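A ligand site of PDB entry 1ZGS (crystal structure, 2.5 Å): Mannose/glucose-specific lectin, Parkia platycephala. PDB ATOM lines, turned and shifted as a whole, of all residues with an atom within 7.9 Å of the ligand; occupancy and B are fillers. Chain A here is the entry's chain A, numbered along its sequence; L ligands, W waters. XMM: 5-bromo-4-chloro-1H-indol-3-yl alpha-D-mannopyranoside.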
ATOM      1  N   GLY A 308       4.420  26.700  20.533  1.00  0.00           N
ATOM      2  CA  GLY A 308       5.849  26.472  20.563  1.00  0.00           C
ATOM      3  C   GLY A 308       6.101  25.031  20.882  1.00  0.00           C
ATOM      4  O   GLY A 308       5.180  24.306  21.259  1.00  0.00           O
ATOM      5  N   SER A 309       7.349  24.603  20.754  1.00  0.00           N
ATOM      6  CA  SER A 309       7.622  23.192  20.867  1.00  0.00           C
ATOM      7  C   SER A 309       8.480  22.875  22.099  1.00  0.00           C
ATOM      8  O   SER A 309       8.888  21.739  22.303  1.00  0.00           O
ATOM      9  CB  SER A 309       8.225  22.669  19.565  1.00  0.00           C
ATOM     10  OG  SER A 309       9.571  23.031  19.528  1.00  0.00           O
ATOM     11  N   GLY A 310       8.719  23.870  22.951  1.00  0.00           N
ATOM     12  CA  GLY A 310       9.241  23.586  24.300  1.00  0.00           C
ATOM     13  C   GLY A 310       8.173  23.163  25.307  1.00  0.00           C
ATOM     14  O   GLY A 310       6.996  22.987  24.965  1.00  0.00           O
ATOM     15  N   GLY A 311       8.582  22.990  26.558  1.00  0.00           N
ATOM     16  CA  GLY A 311       7.673  22.677  27.637  1.00  0.00           C
ATOM     17  C   GLY A 311       7.506  21.194  27.798  1.00  0.00           C
ATOM     18  O   GLY A 311       7.729  20.432  26.844  1.00  0.00           O
ATOM     19  N   ASP A 312       7.148  20.771  29.011  1.00  0.00           N
ATOM     20  CA  ASP A 312       6.829  19.382  29.316  1.00  0.00           C
ATOM     21  C   ASP A 312       5.377  19.038  28.927  1.00  0.00           C
ATOM     22  O   ASP A 312       4.473  19.858  29.138  1.00  0.00           O
ATOM     23  CB  ASP A 312       7.021  19.141  30.803  1.00  0.00           C
ATOM     24  CG  ASP A 312       8.418  19.426  31.271  1.00  0.00           C
ATOM     25  OD1 ASP A 312       9.377  19.066  30.571  1.00  0.00           O
ATOM     26  OD2 ASP A 312       8.672  20.021  32.319  1.00  0.00           O
ATOM     27  N   ASN A 332       2.006  37.370  26.861  1.00  0.00           N
ATOM     28  CA  ASN A 332       1.715  35.984  26.428  1.00  0.00           C
ATOM     29  C   ASN A 332       0.851  35.244  27.454  1.00  0.00           C
ATOM     30  O   ASN A 332       0.261  35.859  28.346  1.00  0.00           O
ATOM     31  CB  ASN A 332       2.995  35.202  26.101  1.00  0.00           C
ATOM     32  CG  ASN A 332       3.781  34.830  27.322  1.00  0.00           C
ATOM     33  OD1 ASN A 332       3.643  35.448  28.375  1.00  0.00           O
ATOM     34  ND2 ASN A 332       4.635  33.798  27.194  1.00  0.00           N
ATOM     35  N   ILE A 333       0.772  33.913  27.352  1.00  0.00           N
ATOM     36  CA  ILE A 333       0.036  33.102  28.299  1.00  0.00           C
ATOM     37  C   ILE A 333       1.021  32.417  29.234  1.00  0.00           C
ATOM     38  O   ILE A 333       1.879  31.663  28.801  1.00  0.00           O
ATOM     39  CB  ILE A 333      -0.879  32.070  27.572  1.00  0.00           C
ATOM     40  CG1 ILE A 333      -1.858  32.783  26.630  1.00  0.00           C
ATOM     41  CG2 ILE A 333      -1.678  31.230  28.557  1.00  0.00           C
ATOM     42  CD1 ILE A 333      -2.814  33.787  27.307  1.00  0.00           C
ATOM     43  N   LYS A 334       0.858  32.669  30.522  1.00  0.00           N
ATOM     44  CA  LYS A 334       1.747  32.120  31.536  1.00  0.00           C
ATOM     45  C   LYS A 334       1.368  30.706  31.999  1.00  0.00           C
ATOM     46  O   LYS A 334       2.242  29.847  32.228  1.00  0.00           O
ATOM     47  CB  LYS A 334       1.728  33.049  32.767  1.00  0.00           C
ATOM     48  CG  LYS A 334       2.751  34.186  32.762  1.00  0.00           C
ATOM     49  CD  LYS A 334       2.473  35.304  31.787  1.00  0.00           C
ATOM     50  CE  LYS A 334       3.797  36.015  31.510  1.00  0.00           C
ATOM     51  NZ  LYS A 334       3.645  37.272  30.786  1.00  0.00           N
ATOM     52  N   GLY A 350       2.114  25.653  33.640  1.00  0.00           N
ATOM     53  CA  GLY A 350       2.842  26.888  33.375  1.00  0.00           C
ATOM     54  C   GLY A 350       2.991  27.706  34.646  1.00  0.00           C
ATOM     55  O   GLY A 350       2.642  27.237  35.722  1.00  0.00           O
ATOM     56  N   GLY A 351       3.519  28.919  34.532  1.00  0.00           N
ATOM     57  CA  GLY A 351       3.641  29.817  35.685  1.00  0.00           C
ATOM     58  C   GLY A 351       4.726  29.428  36.678  1.00  0.00           C
ATOM     59  O   GLY A 351       4.742  29.902  37.806  1.00  0.00           O
ATOM     60  N   VAL A 352       5.635  28.564  36.247  1.00  0.00           N
ATOM     61  CA  VAL A 352       6.744  28.101  37.081  1.00  0.00           C
ATOM     62  C   VAL A 352       7.705  29.237  37.539  1.00  0.00           C
ATOM     63  O   VAL A 352       8.462  29.040  38.496  1.00  0.00           O
ATOM     64  CB  VAL A 352       7.528  26.929  36.345  1.00  0.00           C
ATOM     65  CG1 VAL A 352       8.893  26.651  36.987  1.00  0.00           C
ATOM     66  CG2 VAL A 352       6.666  25.648  36.332  1.00  0.00           C
ATOM     67  N   ASN A 353       7.678  30.400  36.878  1.00  0.00           N
ATOM     68  CA  ASN A 353       8.585  31.503  37.232  1.00  0.00           C
ATOM     69  C   ASN A 353       7.933  32.571  38.094  1.00  0.00           C
ATOM     70  O   ASN A 353       7.138  33.375  37.591  1.00  0.00           O
ATOM     71  CB  ASN A 353       9.147  32.173  35.972  1.00  0.00           C
ATOM     72  CG  ASN A 353      10.354  33.107  36.265  1.00  0.00           C
ATOM     73  OD1 ASN A 353      10.629  33.531  37.421  1.00  0.00           O
ATOM     74  ND2 ASN A 353      11.079  33.472  35.337  1.00  0.00           N
ATOM     75  N   TYR A 382       7.903  35.742  22.605  1.00  0.00           N
ATOM     76  CA  TYR A 382       7.714  36.503  23.820  1.00  0.00           C
ATOM     77  C   TYR A 382       9.063  36.562  24.519  1.00  0.00           C
ATOM     78  O   TYR A 382       9.754  35.532  24.647  1.00  0.00           O
ATOM     79  CB  TYR A 382       6.636  35.867  24.724  1.00  0.00           C
ATOM     80  CG  TYR A 382       6.706  36.407  26.119  1.00  0.00           C
ATOM     81  CD1 TYR A 382       7.528  35.808  27.079  1.00  0.00           C
ATOM     82  CD2 TYR A 382       5.974  37.543  26.498  1.00  0.00           C
ATOM     83  CE1 TYR A 382       7.630  36.322  28.359  1.00  0.00           C
ATOM     84  CE2 TYR A 382       6.066  38.076  27.801  1.00  0.00           C
ATOM     85  CZ  TYR A 382       6.904  37.448  28.709  1.00  0.00           C
ATOM     86  OH  TYR A 382       7.035  37.913  30.001  1.00  0.00           O
ATOM     87  N   LYS A 385      13.703  37.705  29.681  1.00  0.00           N
ATOM     88  CA  LYS A 385      15.128  37.957  29.807  1.00  0.00           C
ATOM     89  C   LYS A 385      15.703  37.262  28.553  1.00  0.00           C
ATOM     90  O   LYS A 385      16.377  37.886  27.718  1.00  0.00           O
ATOM     91  CB  LYS A 385      15.513  37.345  31.149  1.00  0.00           C
ATOM     92  CG  LYS A 385      16.917  37.541  31.692  1.00  0.00           C
ATOM     93  CD  LYS A 385      17.007  36.738  33.023  1.00  0.00           C
ATOM     94  CE  LYS A 385      18.308  35.965  33.091  1.00  0.00           C
ATOM     95  NZ  LYS A 385      19.188  36.427  31.960  1.00  0.00           N
ATOM     96  N   ASP A 386      15.333  35.997  28.410  1.00  0.00           N
ATOM     97  CA  ASP A 386      15.413  35.283  27.138  1.00  0.00           C
ATOM     98  C   ASP A 386      14.177  35.396  26.224  1.00  0.00           C
ATOM     99  O   ASP A 386      13.151  35.976  26.620  1.00  0.00           O
ATOM    100  CB  ASP A 386      15.705  33.832  27.454  1.00  0.00           C
ATOM    101  CG  ASP A 386      17.141  33.633  27.803  1.00  0.00           C
ATOM    102  OD1 ASP A 386      17.487  33.590  29.017  1.00  0.00           O
ATOM    103  OD2 ASP A 386      18.004  33.570  26.902  1.00  0.00           O
ATOM    104  N   VAL A 387      14.306  34.862  25.002  1.00  0.00           N
ATOM    105  CA  VAL A 387      13.211  34.763  24.035  1.00  0.00           C
ATOM    106  C   VAL A 387      12.549  33.374  24.060  1.00  0.00           C
ATOM    107  O   VAL A 387      13.254  32.377  24.166  1.00  0.00           O
ATOM    108  CB  VAL A 387      13.708  35.090  22.594  1.00  0.00           C
ATOM    109  CG1 VAL A 387      13.475  33.910  21.610  1.00  0.00           C
ATOM    110  CG2 VAL A 387      13.081  36.387  22.071  1.00  0.00           C
ATOM    111  N   PHE A 388      11.216  33.326  23.969  1.00  0.00           N
ATOM    112  CA  PHE A 388      10.469  32.045  23.950  1.00  0.00           C
ATOM    113  C   PHE A 388       9.427  32.087  22.877  1.00  0.00           C
ATOM    114  O   PHE A 388       9.005  33.171  22.425  1.00  0.00           O
ATOM    115  CB  PHE A 388       9.749  31.760  25.290  1.00  0.00           C
ATOM    116  CG  PHE A 388      10.596  31.950  26.527  1.00  0.00           C
ATOM    117  CD1 PHE A 388      11.013  33.212  26.936  1.00  0.00           C
ATOM    118  CD2 PHE A 388      10.950  30.868  27.315  1.00  0.00           C
ATOM    119  CE1 PHE A 388      11.789  33.381  28.105  1.00  0.00           C
ATOM    120  CE2 PHE A 388      11.709  31.027  28.484  1.00  0.00           C
ATOM    121  CZ  PHE A 388      12.126  32.266  28.872  1.00  0.00           C
ATOM    122  N   THR A 389       8.981  30.898  22.463  1.00  0.00           N
ATOM    123  CA  THR A 389       7.872  30.765  21.545  1.00  0.00           C
ATOM    124  C   THR A 389       6.736  30.103  22.324  1.00  0.00           C
ATOM    125  O   THR A 389       6.859  28.934  22.718  1.00  0.00           O
ATOM    126  CB  THR A 389       8.354  29.952  20.293  1.00  0.00           C
ATOM    127  OG1 THR A 389       9.401  30.679  19.641  1.00  0.00           O
ATOM    128  CG2 THR A 389       7.270  29.843  19.176  1.00  0.00           C
ATOM    129  N   THR A 390       5.671  30.846  22.598  1.00  0.00           N
ATOM    130  CA  THR A 390       4.549  30.321  23.379  1.00  0.00           C
ATOM    131  C   THR A 390       3.230  30.767  22.823  1.00  0.00           C
ATOM    132  O   THR A 390       3.171  31.561  21.866  1.00  0.00           O
ATOM    133  CB  THR A 390       4.617  30.726  24.871  1.00  0.00           C
ATOM    134  OG1 THR A 390       4.197  32.090  25.020  1.00  0.00           O
ATOM    135  CG2 THR A 390       6.045  30.657  25.436  1.00  0.00           C
ATOM    136  N   ARG A 429       1.794  21.502  26.296  1.00  0.00           N
ATOM    137  CA  ARG A 429       3.131  21.594  26.869  1.00  0.00           C
ATOM    138  C   ARG A 429       3.251  22.916  27.620  1.00  0.00           C
ATOM    139  O   ARG A 429       2.758  23.961  27.157  1.00  0.00           O
ATOM    140  CB  ARG A 429       4.182  21.550  25.747  1.00  0.00           C
ATOM    141  CG  ARG A 429       4.287  20.199  25.033  1.00  0.00           C
ATOM    142  CD  ARG A 429       5.363  20.112  23.916  1.00  0.00           C
ATOM    143  NE  ARG A 429       5.081  21.069  22.853  1.00  0.00           N
ATOM    144  CZ  ARG A 429       4.385  20.804  21.756  1.00  0.00           C
ATOM    145  NH1 ARG A 429       3.900  19.592  21.520  1.00  0.00           N
ATOM    146  NH2 ARG A 429       4.190  21.738  20.843  1.00  0.00           N
ATOM    147  N   ALA A 430       3.905  22.871  28.763  1.00  0.00           N
ATOM    148  CA  ALA A 430       4.097  24.069  29.564  1.00  0.00           C
ATOM    149  C   ALA A 430       5.407  23.958  30.319  1.00  0.00           C
ATOM    150  O   ALA A 430       5.916  22.869  30.554  1.00  0.00           O
ATOM    151  CB  ALA A 430       2.923  24.261  30.554  1.00  0.00           C
ATOM    152  N   GLY A 431       5.942  25.110  30.706  1.00  0.00           N
ATOM    153  CA  GLY A 431       7.166  25.175  31.525  1.00  0.00           C
ATOM    154  C   GLY A 431       6.987  26.440  32.332  1.00  0.00           C
ATOM    155  O   GLY A 431       6.105  26.493  33.191  1.00  0.00           O
ATOM    156  N   ASP A 432       7.788  27.465  32.052  1.00  0.00           N
ATOM    157  CA  ASP A 432       7.539  28.799  32.638  1.00  0.00           C
ATOM    158  C   ASP A 432       6.221  29.388  32.142  1.00  0.00           C
ATOM    159  O   ASP A 432       5.533  30.086  32.885  1.00  0.00           O
ATOM    160  CB  ASP A 432       8.687  29.777  32.340  1.00  0.00           C
ATOM    161  CG  ASP A 432       9.944  29.501  33.192  1.00  0.00           C
ATOM    162  OD1 ASP A 432       9.974  28.522  33.949  1.00  0.00           O
ATOM    163  OD2 ASP A 432      10.952  30.217  33.157  1.00  0.00           O
ATOM    164  N   TYR A 433       5.889  29.100  30.892  1.00  0.00           N
ATOM    165  CA  TYR A 433       4.676  29.577  30.261  1.00  0.00           C
ATOM    166  C   TYR A 433       3.918  28.471  29.524  1.00  0.00           C
ATOM    167  O   TYR A 433       4.291  27.323  29.546  1.00  0.00           O
ATOM    168  CB  TYR A 433       5.028  30.700  29.290  1.00  0.00           C
ATOM    169  CG  TYR A 433       6.083  31.634  29.817  1.00  0.00           C
ATOM    170  CD1 TYR A 433       7.365  31.610  29.307  1.00  0.00           C
ATOM    171  CD2 TYR A 433       5.800  32.529  30.855  1.00  0.00           C
ATOM    172  CE1 TYR A 433       8.351  32.459  29.779  1.00  0.00           C
ATOM    173  CE2 TYR A 433       6.792  33.388  31.348  1.00  0.00           C
ATOM    174  CZ  TYR A 433       8.062  33.343  30.796  1.00  0.00           C
ATOM    175  OH  TYR A 433       9.073  34.166  31.245  1.00  0.00           O
ATOM    176  N   LEU A 434       2.832  28.842  28.857  1.00  0.00           N
ATOM    177  CA  LEU A 434       2.110  27.872  28.079  1.00  0.00           C
ATOM    178  C   LEU A 434       2.657  27.764  26.633  1.00  0.00           C
ATOM    179  O   LEU A 434       2.146  28.423  25.702  1.00  0.00           O
ATOM    180  CB  LEU A 434       0.624  28.204  28.089  1.00  0.00           C
ATOM    181  CG  LEU A 434      -0.297  27.243  27.342  1.00  0.00           C
ATOM    182  CD1 LEU A 434      -0.246  25.870  27.941  1.00  0.00           C
ATOM    183  CD2 LEU A 434      -1.722  27.790  27.311  1.00  0.00           C
ATOM    184  N   ASP A 435       3.671  26.914  26.452  1.00  0.00           N
ATOM    185  CA  ASP A 435       4.230  26.669  25.109  1.00  0.00           C
ATOM    186  C   ASP A 435       3.191  26.282  24.048  1.00  0.00           C
ATOM    187  O   ASP A 435       3.224  26.819  22.931  1.00  0.00           O
ATOM    188  CB  ASP A 435       5.268  25.569  25.183  1.00  0.00           C
ATOM    189  CG  ASP A 435       6.351  25.873  26.141  1.00  0.00           C
ATOM    190  OD1 ASP A 435       7.448  26.302  25.685  1.00  0.00           O
ATOM    191  OD2 ASP A 435       6.161  25.762  27.373  1.00  0.00           O
ATOM    192  N   ALA A 436       2.306  25.328  24.383  1.00  0.00           N
ATOM    193  CA  ALA A 436       1.359  24.803  23.392  1.00  0.00           C
ATOM    194  C   ALA A 436       0.094  24.278  24.045  1.00  0.00           C
ATOM    195  O   ALA A 436       0.139  23.826  25.167  1.00  0.00           O
ATOM    196  CB  ALA A 436       2.013  23.711  22.536  1.00  0.00           C
HETATM  197  O2  XMM L   1       9.860  24.042  29.895  1.00  0.00           O
HETATM  198  C2  XMM L   1      11.065  24.764  29.694  1.00  0.00           C
HETATM  199  C3  XMM L   1      11.119  25.038  28.203  1.00  0.00           C
HETATM  200  O3  XMM L   1      11.100  23.821  27.449  1.00  0.00           O
HETATM  201  C4  XMM L   1       9.867  25.827  27.871  1.00  0.00           C
HETATM  202  O4  XMM L   1       9.849  26.257  26.522  1.00  0.00           O
HETATM  203  C5  XMM L   1       9.705  27.084  28.706  1.00  0.00           C
HETATM  204  O5  XMM L   1       9.972  26.907  30.091  1.00  0.00           O
HETATM  205  C6  XMM L   1       8.215  27.250  28.578  1.00  0.00           C
HETATM  206  O6  XMM L   1       7.811  28.324  29.378  1.00  0.00           O
HETATM  207  C1  XMM L   1      11.076  26.079  30.500  1.00  0.00           C
HETATM  208  O1  XMM L   1      12.329  26.664  30.146  1.00  0.00           O
HETATM  209  C7  XMM L   1      13.108  27.697  30.611  1.00  0.00           C
HETATM  210  C8  XMM L   1      14.024  28.604  29.785  1.00  0.00           C
HETATM  211  C9  XMM L   1      14.628  29.494  30.821  1.00  0.00           C
HETATM  212  N1  XMM L   1      14.172  29.189  32.141  1.00  0.00           N
HETATM  213  C11 XMM L   1      13.405  28.223  31.762  1.00  0.00           C
HETATM  214  C10 XMM L   1      14.338  28.687  28.383  1.00  0.00           C
HETATM  215 CL   XMM L   1      13.679  27.736  27.439  1.00  0.00          CL
HETATM  216  C13 XMM L   1      15.358  29.762  27.951  1.00  0.00           C
HETATM  217 BR   XMM L   1      15.877  30.159  26.652  1.00  0.00          BR
HETATM  218  C14 XMM L   1      15.651  30.312  29.053  1.00  0.00           C
HETATM  219  C12 XMM L   1      15.557  30.463  30.343  1.00  0.00           C
HETATM  220  O   HOH W   1      11.201  21.527  28.670  1.00  0.00           O
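Residues that only touch the ligand: Gly 310 (3.5 Å), Asp 386 (3.8 Å), Phe 388 (3.5 Å) and Gly 431 (3.3 Å).
Hydrophobic or aromatic side chains that line the ligand: Phe 388 and Tyr 433.
Within 4 Å of the ligand: Gly 310, Gly 311, Asp 386, Phe 388, Gly 431, Asp 432, Tyr 433 and Asp 435.
The nearest printed residue that does not touch the ligand is Ala 430 (4.2 Å).
The side-chain carboxylate (OD2) of Asp 435 sits at hydrogen-bond distance from the backbone NH (N) of Gly 431, 3.4 Å away.
The backbone carbonyl oxygen (O) of Arg 429 lies within hydrogen-bond range of the backbone NH (N) of Asp 435, at 3.2 Å.
O of Asp 435 is in hydrogen-bond range of N of Gly 308 (2.7 Å).
The backbone NH (N) of Gly 351 is in hydrogen-bond range of the backbone carbonyl oxygen (O) of Asp 432 (2.9 Å).
N of Phe 388 lies within hydrogen-bond range of O of Tyr 382 (2.7 Å).
The guanidinium group (NE) of Arg 429 sits close to the backbone carbonyl oxygen (O) of Gly 310, 3.4 Å away.
OD1 of Asp 435 lies within hydrogen-bond range of O4 of the ligand (2.5 Å).
The backbone NH of Tyr 433 is in hydrogen-bond range of an oxygen (O6) of the ligand (2.6 Å).
An oxygen (O3) of the ligand lies within hydrogen-bond range of the backbone NH (N) of Gly 311.
The backbone NH (N) of Asp 432 lies within hydrogen-bond range of an oxygen (O6) of the ligand (2.8 Å).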
